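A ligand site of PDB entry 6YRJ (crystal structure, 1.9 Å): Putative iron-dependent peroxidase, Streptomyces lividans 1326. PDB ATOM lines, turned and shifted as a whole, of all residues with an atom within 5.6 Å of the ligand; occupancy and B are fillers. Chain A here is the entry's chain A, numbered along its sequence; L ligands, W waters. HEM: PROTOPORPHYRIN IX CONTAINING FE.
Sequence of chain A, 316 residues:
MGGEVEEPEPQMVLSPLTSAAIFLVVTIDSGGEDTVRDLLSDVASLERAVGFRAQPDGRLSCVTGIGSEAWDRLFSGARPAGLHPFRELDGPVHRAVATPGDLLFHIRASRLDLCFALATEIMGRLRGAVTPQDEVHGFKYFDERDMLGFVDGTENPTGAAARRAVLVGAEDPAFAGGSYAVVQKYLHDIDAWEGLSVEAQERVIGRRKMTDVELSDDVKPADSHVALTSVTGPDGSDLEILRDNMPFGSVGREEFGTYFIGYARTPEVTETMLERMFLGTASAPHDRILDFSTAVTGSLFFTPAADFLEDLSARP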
ATOM      1  N   ASP A 146      -6.947 -21.023   2.952  1.00  0.00           N
ATOM      2  CA  ASP A 146      -6.883 -21.697   4.260  1.00  0.00           C
ATOM      3  C   ASP A 146      -7.945 -21.083   5.140  1.00  0.00           C
ATOM      4  O   ASP A 146      -8.737 -20.211   4.693  1.00  0.00           O
ATOM      5  CB  ASP A 146      -5.465 -21.639   4.826  1.00  0.00           C
ATOM      6  CG  ASP A 146      -4.900 -20.271   5.061  1.00  0.00           C
ATOM      7  OD1 ASP A 146      -5.710 -19.348   5.320  1.00  0.00           O
ATOM      8  OD2 ASP A 146      -3.654 -20.138   4.918  1.00  0.00           O
ATOM      9  N   LEU A 148      -7.804 -18.957   7.378  1.00  0.00           N
ATOM     10  CA  LEU A 148      -7.681 -17.491   7.582  1.00  0.00           C
ATOM     11  C   LEU A 148      -8.194 -16.712   6.358  1.00  0.00           C
ATOM     12  O   LEU A 148      -8.247 -15.471   6.459  1.00  0.00           O
ATOM     13  CB  LEU A 148      -6.246 -17.121   7.883  1.00  0.00           C
ATOM     14  CG  LEU A 148      -5.642 -17.857   9.088  1.00  0.00           C
ATOM     15  CD1 LEU A 148      -4.201 -17.414   9.309  1.00  0.00           C
ATOM     16  CD2 LEU A 148      -6.498 -17.638  10.315  1.00  0.00           C
ATOM     17  N   PHE A 150      -6.860 -16.712   3.344  1.00  0.00           N
ATOM     18  CA  PHE A 150      -5.732 -16.433   2.424  1.00  0.00           C
ATOM     19  C   PHE A 150      -5.427 -17.657   1.587  1.00  0.00           C
ATOM     20  O   PHE A 150      -5.508 -18.802   2.044  1.00  0.00           O
ATOM     21  CB  PHE A 150      -4.518 -15.929   3.199  1.00  0.00           C
ATOM     22  CG  PHE A 150      -4.645 -14.481   3.596  1.00  0.00           C
ATOM     23  CD1 PHE A 150      -5.460 -14.107   4.648  1.00  0.00           C
ATOM     24  CD2 PHE A 150      -3.878 -13.521   2.976  1.00  0.00           C
ATOM     25  CE1 PHE A 150      -5.594 -12.779   5.008  1.00  0.00           C
ATOM     26  CE2 PHE A 150      -3.986 -12.206   3.359  1.00  0.00           C
ATOM     27  CZ  PHE A 150      -4.848 -11.823   4.358  1.00  0.00           C
ATOM     28  N   VAL A 151      -5.056 -17.375   0.334  1.00  0.00           N
ATOM     29  CA  VAL A 151      -4.563 -18.421  -0.608  1.00  0.00           C
ATOM     30  C   VAL A 151      -3.295 -18.970   0.023  1.00  0.00           C
ATOM     31  O   VAL A 151      -2.458 -18.186   0.511  1.00  0.00           O
ATOM     32  CB  VAL A 151      -4.329 -17.889  -2.035  1.00  0.00           C
ATOM     33  CG1 VAL A 151      -3.852 -19.018  -2.945  1.00  0.00           C
ATOM     34  CG2 VAL A 151      -5.597 -17.204  -2.606  1.00  0.00           C
ATOM     35  N   ASP A 152      -3.182 -20.282   0.026  1.00  0.00           N
ATOM     36  CA  ASP A 152      -2.129 -20.977   0.786  1.00  0.00           C
ATOM     37  C   ASP A 152      -1.478 -22.007  -0.139  1.00  0.00           C
ATOM     38  O   ASP A 152      -2.167 -22.933  -0.556  1.00  0.00           O
ATOM     39  CB  ASP A 152      -2.776 -21.577   2.029  1.00  0.00           C
ATOM     40  CG  ASP A 152      -1.803 -22.028   3.084  1.00  0.00           C
ATOM     41  OD1 ASP A 152      -0.740 -22.541   2.726  1.00  0.00           O
ATOM     42  OD2 ASP A 152      -2.132 -21.864   4.277  1.00  0.00           O
ATOM     43  N   GLY A 153      -0.250 -21.772  -0.536  1.00  0.00           N
ATOM     44  CA  GLY A 153       0.551 -22.665  -1.378  1.00  0.00           C
ATOM     45  C   GLY A 153       1.275 -21.902  -2.471  1.00  0.00           C
ATOM     46  O   GLY A 153       2.141 -22.481  -3.127  1.00  0.00           O
ATOM     47  N   THR A 154       0.897 -20.648  -2.659  1.00  0.00           N
ATOM     48  CA  THR A 154       1.290 -19.820  -3.809  1.00  0.00           C
ATOM     49  C   THR A 154       2.799 -19.859  -4.044  1.00  0.00           C
ATOM     50  O   THR A 154       3.177 -20.098  -5.202  1.00  0.00           O
ATOM     51  CB  THR A 154       0.884 -18.369  -3.613  1.00  0.00           C
ATOM     52  OG1 THR A 154      -0.487 -18.358  -3.217  1.00  0.00           O
ATOM     53  CG2 THR A 154       1.067 -17.552  -4.875  1.00  0.00           C
ATOM     54  N   GLU A 155       3.617 -19.637  -3.035  1.00  0.00           N
ATOM     55  CA  GLU A 155       5.078 -19.547  -3.246  1.00  0.00           C
ATOM     56  C   GLU A 155       5.791 -20.895  -3.025  1.00  0.00           C
ATOM     57  O   GLU A 155       7.034 -20.873  -3.020  1.00  0.00           O
ATOM     58  CB  GLU A 155       5.666 -18.412  -2.413  1.00  0.00           C
ATOM     59  CG  GLU A 155       5.268 -17.060  -2.964  1.00  0.00           C
ATOM     60  CD  GLU A 155       5.829 -16.808  -4.344  1.00  0.00           C
ATOM     61  OE1 GLU A 155       7.034 -16.912  -4.476  1.00  0.00           O
ATOM     62  OE2 GLU A 155       5.055 -16.623  -5.293  1.00  0.00           O
ATOM     63  N   ASN A 156       5.079 -22.001  -2.960  1.00  0.00           N
ATOM     64  CA  ASN A 156       5.740 -23.328  -2.949  1.00  0.00           C
ATOM     65  C   ASN A 156       6.637 -23.432  -4.178  1.00  0.00           C
ATOM     66  O   ASN A 156       6.240 -23.108  -5.284  1.00  0.00           O
ATOM     67  CB  ASN A 156       4.779 -24.504  -3.004  1.00  0.00           C
ATOM     68  CG  ASN A 156       4.361 -24.960  -1.635  1.00  0.00           C
ATOM     69  OD1 ASN A 156       5.181 -24.914  -0.726  1.00  0.00           O
ATOM     70  ND2 ASN A 156       3.113 -25.437  -1.503  1.00  0.00           N
ATOM     71  N   GLN A 184       2.750 -29.687  12.264  1.00  0.00           N
ATOM     72  CA  GLN A 184       2.200 -29.003  13.441  1.00  0.00           C
ATOM     73  C   GLN A 184       0.704 -28.804  13.189  1.00  0.00           C
ATOM     74  O   GLN A 184       0.385 -28.264  12.130  1.00  0.00           O
ATOM     75  CB  GLN A 184       2.836 -27.639  13.621  1.00  0.00           C
ATOM     76  CG  GLN A 184       4.322 -27.659  13.980  1.00  0.00           C
ATOM     77  CD  GLN A 184       4.742 -26.213  14.108  1.00  0.00           C
ATOM     78  OE1 GLN A 184       4.740 -25.457  13.127  1.00  0.00           O
ATOM     79  NE2 GLN A 184       5.005 -25.757  15.339  1.00  0.00           N
ATOM     80  N   TYR A 186      -2.266 -26.594  13.925  1.00  0.00           N
ATOM     81  CA  TYR A 186      -2.599 -25.257  14.456  1.00  0.00           C
ATOM     82  C   TYR A 186      -4.115 -25.128  14.606  1.00  0.00           C
ATOM     83  O   TYR A 186      -4.849 -25.525  13.672  1.00  0.00           O
ATOM     84  CB  TYR A 186      -2.070 -24.149  13.553  1.00  0.00           C
ATOM     85  CG  TYR A 186      -0.587 -23.948  13.622  1.00  0.00           C
ATOM     86  CD1 TYR A 186      -0.061 -23.062  14.529  1.00  0.00           C
ATOM     87  CD2 TYR A 186       0.276 -24.592  12.740  1.00  0.00           C
ATOM     88  CE1 TYR A 186       1.288 -22.801  14.582  1.00  0.00           C
ATOM     89  CE2 TYR A 186       1.646 -24.371  12.816  1.00  0.00           C
ATOM     90  CZ  TYR A 186       2.147 -23.460  13.734  1.00  0.00           C
ATOM     91  OH  TYR A 186       3.481 -23.139  13.805  1.00  0.00           O
ATOM     92  N   HIS A 188      -6.884 -21.986  15.135  1.00  0.00           N
ATOM     93  CA  HIS A 188      -6.949 -20.535  14.933  1.00  0.00           C
ATOM     94  C   HIS A 188      -8.019 -19.941  15.824  1.00  0.00           C
ATOM     95  O   HIS A 188      -9.043 -20.544  16.031  1.00  0.00           O
ATOM     96  CB  HIS A 188      -7.250 -20.182  13.472  1.00  0.00           C
ATOM     97  CG  HIS A 188      -6.194 -20.650  12.531  1.00  0.00           C
ATOM     98  ND1 HIS A 188      -4.933 -20.121  12.534  1.00  0.00           N
ATOM     99  CD2 HIS A 188      -6.245 -21.565  11.542  1.00  0.00           C
ATOM    100  CE1 HIS A 188      -4.213 -20.740  11.595  1.00  0.00           C
ATOM    101  NE2 HIS A 188      -5.006 -21.607  10.956  1.00  0.00           N
ATOM    102  N   ILE A 205      -0.110 -11.315   7.178  1.00  0.00           N
ATOM    103  CA  ILE A 205       0.342 -12.376   6.251  1.00  0.00           C
ATOM    104  C   ILE A 205       1.498 -11.829   5.383  1.00  0.00           C
ATOM    105  O   ILE A 205       2.517 -12.519   5.275  1.00  0.00           O
ATOM    106  CB  ILE A 205      -0.818 -12.894   5.397  1.00  0.00           C
ATOM    107  CG1 ILE A 205      -1.930 -13.477   6.265  1.00  0.00           C
ATOM    108  CG2 ILE A 205      -0.315 -13.853   4.340  1.00  0.00           C
ATOM    109  CD1 ILE A 205      -1.553 -14.729   6.979  1.00  0.00           C
ATOM    110  N   ARG A 207       0.609 -10.536   2.150  1.00  0.00           N
ATOM    111  CA  ARG A 207       0.036 -10.606   0.799  1.00  0.00           C
ATOM    112  C   ARG A 207      -1.363 -10.007   0.869  1.00  0.00           C
ATOM    113  O   ARG A 207      -1.951 -10.011   1.969  1.00  0.00           O
ATOM    114  CB  ARG A 207       0.015 -12.047   0.287  1.00  0.00           C
ATOM    115  CG  ARG A 207       1.320 -12.807   0.442  1.00  0.00           C
ATOM    116  CD  ARG A 207       1.262 -14.205  -0.116  1.00  0.00           C
ATOM    117  NE  ARG A 207       1.114 -14.187  -1.577  1.00  0.00           N
ATOM    118  CZ  ARG A 207       2.116 -14.167  -2.442  1.00  0.00           C
ATOM    119  NH1 ARG A 207       3.360 -14.277  -2.024  1.00  0.00           N
ATOM    120  NH2 ARG A 207       1.864 -14.071  -3.732  1.00  0.00           N
ATOM    121  N   ASP A 212      -4.001 -12.040  -3.768  1.00  0.00           N
ATOM    122  CA  ASP A 212      -2.814 -12.884  -3.446  1.00  0.00           C
ATOM    123  C   ASP A 212      -1.542 -12.334  -4.084  1.00  0.00           C
ATOM    124  O   ASP A 212      -0.599 -13.121  -4.376  1.00  0.00           O
ATOM    125  CB  ASP A 212      -3.020 -14.323  -3.889  1.00  0.00           C
ATOM    126  CG  ASP A 212      -2.008 -15.280  -3.292  1.00  0.00           C
ATOM    127  OD1 ASP A 212      -1.408 -14.921  -2.224  1.00  0.00           O
ATOM    128  OD2 ASP A 212      -1.865 -16.361  -3.861  1.00  0.00           O
ATOM    129  N   GLU A 214       1.861 -10.302  -3.440  1.00  0.00           N
ATOM    130  CA  GLU A 214       2.742  -9.979  -2.305  1.00  0.00           C
ATOM    131  C   GLU A 214       2.763  -8.459  -2.104  1.00  0.00           C
ATOM    132  O   GLU A 214       2.682  -7.731  -3.123  1.00  0.00           O
ATOM    133  CB  GLU A 214       4.127 -10.556  -2.583  1.00  0.00           C
ATOM    134  CG  GLU A 214       5.082 -10.332  -1.442  1.00  0.00           C
ATOM    135  CD  GLU A 214       6.360 -11.144  -1.606  1.00  0.00           C
ATOM    136  OE1 GLU A 214       6.479 -11.800  -2.637  1.00  0.00           O
ATOM    137  OE2 GLU A 214       7.188 -11.100  -0.703  1.00  0.00           O
ATOM    138  N   HIS A 225       4.127 -12.745   8.212  1.00  0.00           N
ATOM    139  CA  HIS A 225       4.425 -14.170   8.030  1.00  0.00           C
ATOM    140  C   HIS A 225       5.412 -14.385   6.888  1.00  0.00           C
ATOM    141  O   HIS A 225       6.422 -15.145   7.073  1.00  0.00           O
ATOM    142  CB  HIS A 225       3.106 -14.907   7.825  1.00  0.00           C
ATOM    143  CG  HIS A 225       3.337 -16.366   7.732  1.00  0.00           C
ATOM    144  ND1 HIS A 225       3.995 -17.076   8.702  1.00  0.00           N
ATOM    145  CD2 HIS A 225       3.012 -17.234   6.757  1.00  0.00           C
ATOM    146  CE1 HIS A 225       4.053 -18.341   8.341  1.00  0.00           C
ATOM    147  NE2 HIS A 225       3.451 -18.474   7.144  1.00  0.00           N
ATOM    148  N   VAL A 226       5.122 -13.790   5.733  1.00  0.00           N
ATOM    149  CA  VAL A 226       5.961 -13.964   4.523  1.00  0.00           C
ATOM    150  C   VAL A 226       7.358 -13.364   4.786  1.00  0.00           C
ATOM    151  O   VAL A 226       8.353 -13.948   4.344  1.00  0.00           O
ATOM    152  CB  VAL A 226       5.274 -13.349   3.296  1.00  0.00           C
ATOM    153  CG1 VAL A 226       6.220 -13.183   2.131  1.00  0.00           C
ATOM    154  CG2 VAL A 226       4.099 -14.228   2.886  1.00  0.00           C
ATOM    155  N   THR A 229       9.295 -15.994   7.144  1.00  0.00           N
ATOM    156  CA  THR A 229       9.558 -17.317   6.540  1.00  0.00           C
ATOM    157  C   THR A 229      10.315 -17.172   5.224  1.00  0.00           C
ATOM    158  O   THR A 229      10.489 -18.205   4.564  1.00  0.00           O
ATOM    159  CB  THR A 229       8.249 -18.107   6.398  1.00  0.00           C
ATOM    160  OG1 THR A 229       7.392 -17.378   5.525  1.00  0.00           O
ATOM    161  CG2 THR A 229       7.619 -18.332   7.741  1.00  0.00           C
ATOM    162  N   SER A 230      10.684 -15.955   4.819  1.00  0.00           N
ATOM    163  CA  SER A 230      11.632 -15.719   3.696  1.00  0.00           C
ATOM    164  C   SER A 230      13.044 -15.746   4.255  1.00  0.00           C
ATOM    165  O   SER A 230      13.364 -14.888   5.079  1.00  0.00           O
ATOM    166  CB  SER A 230      11.352 -14.405   3.004  1.00  0.00           C
ATOM    167  OG  SER A 230      10.121 -14.485   2.341  1.00  0.00           O
ATOM    168  N   ILE A 241      10.992 -24.518   1.385  1.00  0.00           N
ATOM    169  CA  ILE A 241      10.348 -25.787   1.790  1.00  0.00           C
ATOM    170  C   ILE A 241       9.116 -25.984   0.916  1.00  0.00           C
ATOM    171  O   ILE A 241       8.622 -25.023   0.314  1.00  0.00           O
ATOM    172  CB  ILE A 241       9.989 -25.783   3.285  1.00  0.00           C
ATOM    173  CG1 ILE A 241       8.909 -24.750   3.623  1.00  0.00           C
ATOM    174  CG2 ILE A 241      11.230 -25.565   4.148  1.00  0.00           C
ATOM    175  CD1 ILE A 241       8.429 -24.860   5.054  1.00  0.00           C
ATOM    176  N   ARG A 243       5.276 -27.002   1.251  1.00  0.00           N
ATOM    177  CA  ARG A 243       4.150 -27.103   2.185  1.00  0.00           C
ATOM    178  C   ARG A 243       2.943 -27.718   1.484  1.00  0.00           C
ATOM    179  O   ARG A 243       2.720 -27.499   0.226  1.00  0.00           O
ATOM    180  CB  ARG A 243       3.790 -25.711   2.700  1.00  0.00           C
ATOM    181  CG  ARG A 243       4.860 -25.091   3.575  1.00  0.00           C
ATOM    182  CD  ARG A 243       4.517 -23.631   3.791  1.00  0.00           C
ATOM    183  NE  ARG A 243       4.715 -22.917   2.540  1.00  0.00           N
ATOM    184  CZ  ARG A 243       3.804 -22.171   1.908  1.00  0.00           C
ATOM    185  NH1 ARG A 243       2.592 -22.031   2.422  1.00  0.00           N
ATOM    186  NH2 ARG A 243       4.102 -21.577   0.762  1.00  0.00           N
ATOM    187  N   ASN A 245      -0.310 -27.319   3.437  1.00  0.00           N
ATOM    188  CA  ASN A 245      -1.163 -26.933   4.574  1.00  0.00           C
ATOM    189  C   ASN A 245      -2.603 -27.331   4.273  1.00  0.00           C
ATOM    190  O   ASN A 245      -3.086 -27.055   3.140  1.00  0.00           O
ATOM    191  CB  ASN A 245      -1.136 -25.437   4.827  1.00  0.00           C
ATOM    192  CG  ASN A 245       0.189 -24.982   5.380  1.00  0.00           C
ATOM    193  OD1 ASN A 245       1.023 -25.829   5.684  1.00  0.00           O
ATOM    194  ND2 ASN A 245       0.400 -23.678   5.445  1.00  0.00           N
ATOM    195  N   THR A 258      -5.421 -25.244  10.842  1.00  0.00           N
ATOM    196  CA  THR A 258      -4.504 -25.432   9.699  1.00  0.00           C
ATOM    197  C   THR A 258      -3.596 -26.574  10.110  1.00  0.00           C
ATOM    198  O   THR A 258      -2.932 -26.448  11.130  1.00  0.00           O
ATOM    199  CB  THR A 258      -3.681 -24.201   9.317  1.00  0.00           C
ATOM    200  OG1 THR A 258      -4.635 -23.201   8.925  1.00  0.00           O
ATOM    201  CG2 THR A 258      -2.715 -24.462   8.174  1.00  0.00           C
ATOM    202  N   PHE A 260      -0.324 -27.925   9.371  1.00  0.00           N
ATOM    203  CA  PHE A 260       0.938 -27.588   8.695  1.00  0.00           C
ATOM    204  C   PHE A 260       1.742 -28.862   8.435  1.00  0.00           C
ATOM    205  O   PHE A 260       1.976 -29.606   9.360  1.00  0.00           O
ATOM    206  CB  PHE A 260       1.768 -26.595   9.505  1.00  0.00           C
ATOM    207  CG  PHE A 260       3.138 -26.402   8.951  1.00  0.00           C
ATOM    208  CD1 PHE A 260       3.367 -25.569   7.882  1.00  0.00           C
ATOM    209  CD2 PHE A 260       4.214 -27.074   9.503  1.00  0.00           C
ATOM    210  CE1 PHE A 260       4.655 -25.384   7.388  1.00  0.00           C
ATOM    211  CE2 PHE A 260       5.486 -26.908   8.991  1.00  0.00           C
ATOM    212  CZ  PHE A 260       5.701 -26.059   7.934  1.00  0.00           C
ATOM    213  N   THR A 270      13.586 -25.850   7.781  1.00  0.00           N
ATOM    214  CA  THR A 270      12.264 -25.717   8.458  1.00  0.00           C
ATOM    215  C   THR A 270      12.438 -25.142   9.856  1.00  0.00           C
ATOM    216  O   THR A 270      11.650 -24.277  10.271  1.00  0.00           O
ATOM    217  CB  THR A 270      11.541 -27.058   8.507  1.00  0.00           C
ATOM    218  OG1 THR A 270      11.684 -27.669   7.230  1.00  0.00           O
ATOM    219  CG2 THR A 270      10.072 -26.891   8.810  1.00  0.00           C
ATOM    220  N   MET A 273      13.121 -21.372   9.959  1.00  0.00           N
ATOM    221  CA  MET A 273      11.823 -20.670   9.775  1.00  0.00           C
ATOM    222  C   MET A 273      11.067 -20.715  11.087  1.00  0.00           C
ATOM    223  O   MET A 273      10.564 -19.640  11.498  1.00  0.00           O
ATOM    224  CB  MET A 273      11.030 -21.318   8.666  1.00  0.00           C
ATOM    225  CG  MET A 273      11.688 -21.170   7.328  1.00  0.00           C
ATOM    226  SD  MET A 273      10.711 -21.976   6.071  1.00  0.00           S
ATOM    227  CE  MET A 273      11.608 -21.478   4.610  1.00  0.00           C
ATOM    228  N   LEU A 274      10.972 -21.884  11.727  1.00  0.00           N
ATOM    229  CA  LEU A 274      10.226 -21.972  13.011  1.00  0.00           C
ATOM    230  C   LEU A 274      10.858 -21.066  14.072  1.00  0.00           C
ATOM    231  O   LEU A 274      10.113 -20.461  14.848  1.00  0.00           O
ATOM    232  CB  LEU A 274      10.179 -23.419  13.515  1.00  0.00           C
ATOM    233  CG  LEU A 274       9.239 -24.344  12.777  1.00  0.00           C
ATOM    234  CD1 LEU A 274       9.464 -25.786  13.216  1.00  0.00           C
ATOM    235  CD2 LEU A 274       7.796 -23.915  13.022  1.00  0.00           C
ATOM    236  N   MET A 277       9.879 -17.574  13.475  1.00  0.00           N
ATOM    237  CA  MET A 277       8.443 -17.355  13.780  1.00  0.00           C
ATOM    238  C   MET A 277       8.236 -17.212  15.289  1.00  0.00           C
ATOM    239  O   MET A 277       7.476 -16.280  15.711  1.00  0.00           O
ATOM    240  CB  MET A 277       7.594 -18.509  13.232  1.00  0.00           C
ATOM    241  CG  MET A 277       7.553 -18.509  11.717  1.00  0.00           C
ATOM    242  SD  MET A 277       6.605 -19.903  11.132  1.00  0.00           S
ATOM    243  CE  MET A 277       5.060 -19.636  11.988  1.00  0.00           C
ATOM    244  N   ILE A 289       1.207 -14.114  12.659  1.00  0.00           N
ATOM    245  CA  ILE A 289       0.257 -15.236  12.426  1.00  0.00           C
ATOM    246  C   ILE A 289       0.032 -16.004  13.721  1.00  0.00           C
ATOM    247  O   ILE A 289      -1.041 -16.512  13.922  1.00  0.00           O
ATOM    248  CB  ILE A 289       0.702 -16.124  11.247  1.00  0.00           C
ATOM    249  CG1 ILE A 289      -0.510 -16.723  10.517  1.00  0.00           C
ATOM    250  CG2 ILE A 289       1.676 -17.221  11.656  1.00  0.00           C
ATOM    251  CD1 ILE A 289      -0.143 -17.475   9.280  1.00  0.00           C
ATOM    252  N   LEU A 290       1.032 -16.097  14.605  1.00  0.00           N
ATOM    253  CA  LEU A 290       0.904 -16.858  15.864  1.00  0.00           C
ATOM    254  C   LEU A 290       0.019 -16.149  16.879  1.00  0.00           C
ATOM    255  O   LEU A 290      -0.410 -16.829  17.793  1.00  0.00           O
ATOM    256  CB  LEU A 290       2.295 -17.119  16.447  1.00  0.00           C
ATOM    257  CG  LEU A 290       3.222 -17.896  15.530  1.00  0.00           C
ATOM    258  CD1 LEU A 290       4.647 -17.897  16.067  1.00  0.00           C
ATOM    259  CD2 LEU A 290       2.714 -19.318  15.302  1.00  0.00           C
ATOM    260  N   SER A 293      -2.980 -18.122  15.991  1.00  0.00           N
ATOM    261  CA  SER A 293      -2.711 -19.531  15.635  1.00  0.00           C
ATOM    262  C   SER A 293      -1.956 -20.177  16.771  1.00  0.00           C
ATOM    263  O   SER A 293      -0.859 -19.692  17.102  1.00  0.00           O
ATOM    264  CB  SER A 293      -1.961 -19.658  14.353  1.00  0.00           C
ATOM    265  OG  SER A 293      -2.509 -18.851  13.343  1.00  0.00           O
HETATM  266  CHA HEM L   1       3.584 -18.672   3.066  1.00  0.00           C
HETATM  267  CHB HEM L   1      -0.252 -19.626   5.789  1.00  0.00           C
HETATM  268  CHC HEM L   1       2.505 -21.902   9.037  1.00  0.00           C
HETATM  269  CHD HEM L   1       6.263 -21.359   6.038  1.00  0.00           C
HETATM  270  C1A HEM L   1       2.318 -18.710   3.557  1.00  0.00           C
HETATM  271  C2A HEM L   1       1.232 -18.027   2.970  1.00  0.00           C
HETATM  272  C3A HEM L   1       0.155 -18.284   3.741  1.00  0.00           C
HETATM  273  C4A HEM L   1       0.546 -19.158   4.785  1.00  0.00           C
HETATM  274  CMA HEM L   1      -1.261 -17.790   3.520  1.00  0.00           C
HETATM  275  CAA HEM L   1       1.253 -17.105   1.768  1.00  0.00           C
HETATM  276  CBA HEM L   1       1.017 -17.743   0.419  1.00  0.00           C
HETATM  277  CGA HEM L   1       1.958 -18.883   0.207  1.00  0.00           C
HETATM  278  O1A HEM L   1       1.661 -20.025   0.592  1.00  0.00           O
HETATM  279  O2A HEM L   1       3.008 -18.633  -0.404  1.00  0.00           O
HETATM  280  C1B HEM L   1       0.168 -20.342   6.895  1.00  0.00           C
HETATM  281  C2B HEM L   1      -0.708 -20.748   7.948  1.00  0.00           C
HETATM  282  C3B HEM L   1       0.021 -21.419   8.852  1.00  0.00           C
HETATM  283  C4B HEM L   1       1.424 -21.348   8.395  1.00  0.00           C
HETATM  284  CMB HEM L   1      -2.202 -20.593   8.053  1.00  0.00           C
HETATM  285  CAB HEM L   1      -0.582 -21.855  10.140  1.00  0.00           C
HETATM  286  CBB HEM L   1      -0.052 -21.413  11.213  1.00  0.00           C
HETATM  287  C1C HEM L   1       3.779 -21.966   8.527  1.00  0.00           C
HETATM  288  C2C HEM L   1       4.934 -22.575   9.147  1.00  0.00           C
HETATM  289  C3C HEM L   1       6.030 -22.420   8.282  1.00  0.00           C
HETATM  290  C4C HEM L   1       5.509 -21.693   7.149  1.00  0.00           C
HETATM  291  CMC HEM L   1       4.842 -23.259  10.495  1.00  0.00           C
HETATM  292  CAC HEM L   1       7.449 -22.847   8.400  1.00  0.00           C
HETATM  293  CBC HEM L   1       7.956 -23.518   9.371  1.00  0.00           C
HETATM  294  C1D HEM L   1       5.788 -20.619   4.971  1.00  0.00           C
HETATM  295  C2D HEM L   1       6.637 -20.280   3.858  1.00  0.00           C
HETATM  296  C3D HEM L   1       5.910 -19.495   3.002  1.00  0.00           C
HETATM  297  C4D HEM L   1       4.603 -19.379   3.668  1.00  0.00           C
HETATM  298  CMD HEM L   1       8.035 -20.696   3.652  1.00  0.00           C
HETATM  299  CAD HEM L   1       6.347 -18.894   1.699  1.00  0.00           C
HETATM  300  CBD HEM L   1       7.042 -17.565   2.066  1.00  0.00           C
HETATM  301  CGD HEM L   1       7.619 -16.939   0.820  1.00  0.00           C
HETATM  302  O1D HEM L   1       8.704 -17.281   0.420  1.00  0.00           O
HETATM  303  O2D HEM L   1       6.960 -16.190   0.094  1.00  0.00           O
HETATM  304  NA  HEM L   1       1.883 -19.401   4.685  1.00  0.00           N
HETATM  305  NB  HEM L   1       1.419 -20.745   7.192  1.00  0.00           N
HETATM  306  NC  HEM L   1       4.145 -21.469   7.324  1.00  0.00           N
HETATM  307  ND  HEM L   1       4.557 -20.067   4.850  1.00  0.00           N
HETATM  308 FE   HEM L   1       3.058 -20.197   6.105  1.00  0.00          FE
HETATM  309  O   HOH W   1      10.226 -19.002   1.669  1.00  0.00           O
HETATM  310  O   HOH W   2       4.173 -16.119   0.116  1.00  0.00           O
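OD2 of Asp 146 touches CMB of the ligand, 3.5 Å away. Leu 148 touches the ligand (CD1 to CMB, 3.96 Å). Phe 150 touches the ligand. Val 151 touches the ligand (O to CMA, 3.3 Å). Asp 152 touches the ligand (OD2 to CHB, 3.3 Å). Gln 184 touches the ligand (OE1 to CMC, 3.4 Å). Tyr 186 touches the ligand (CG to CBB, 3.5 Å). Arg 207 touches the ligand (CD to CAA, 3.5 Å). Val 226 touches the ligand (CG1 to O2D, 3.7 Å). OG1 of Thr 229 touches C2D of the ligand, at 3.4 Å. Ser 230 touches the ligand (OG to O1D, 3.7 Å). Asn 245 touches the ligand (ND2 to NB, 3.6 Å). OG1 of Thr 258 touches CMB of the ligand, 3.7 Å away. CE1 of Phe 260 touches C2C of the ligand, at 3.3 Å. Thr 270 touches the ligand. Met 273 touches the ligand (CE to CMD, 3.8 Å). Leu 274 touches the ligand (CD2 to CBC, 3.7 Å). SD of Met 277 touches C2C of the ligand (3.7 Å). Ile 289 touches the ligand. Of the 32 residues printed, 24 come within 4 Å of the ligand. The nearest printed residue that does not touch the ligand is Ile 241 (4.03 Å).
Water W1 bridges O1D of the ligand (2.6 Å) and O of Thr 229 (3.0 Å). Water W2 bridges O2D of the ligand (2.8 Å) and NH1 of Arg 207 (2.9 Å).
The backbone carbonyl oxygen of Val 226 is in hydrogen-bond range of the side-chain hydroxyl of Ser 230, at 2.7 Å. The backbone NH (N) of Val 226 lies within hydrogen-bond range of the backbone carbonyl oxygen (O) of Ile 205, at 2.9 Å. The side-chain carboxylate (OD1) of Asp 146 sits at hydrogen-bond distance from the backbone NH (N) of Phe 150, at 3.5 Å. The side-chain carboxylate (OD1) of Asp 146 is in hydrogen-bond range of the backbone NH (N) of Leu 148, 3.0 Å away. OH of Tyr 186 lies within hydrogen-bond range of OE1 of Gln 184 (2.7 Å). The backbone carbonyl oxygen (O) of Arg 243 lies within hydrogen-bond range of the side-chain amide nitrogen (ND2) of Asn 156 (2.7 Å). The backbone carbonyl oxygen of Ile 289 lies within hydrogen-bond range of the side-chain hydroxyl of Ser 293. The side-chain carboxylate (OD2) of Asp 212 is in hydrogen-bond range of the side-chain hydroxyl (OG1) of Thr 154.
An oxygen (O1A) of the ligand sits at hydrogen-bond distance from the backbone NH of Thr 154 (3.4 Å). An oxygen (O1A) of the ligand is in hydrogen-bond range of the backbone NH (N) of Gly 153 (2.8 Å). N of Glu 155 lies within hydrogen-bond range of O2A of the ligand (2.9 Å). O1A of the ligand is in salt-bridge range of NH1 of Arg 243 (2.9 Å). A ring nitrogen (NE2) of His 225 binds an iron atom (FE) of the ligand (2.1 Å).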
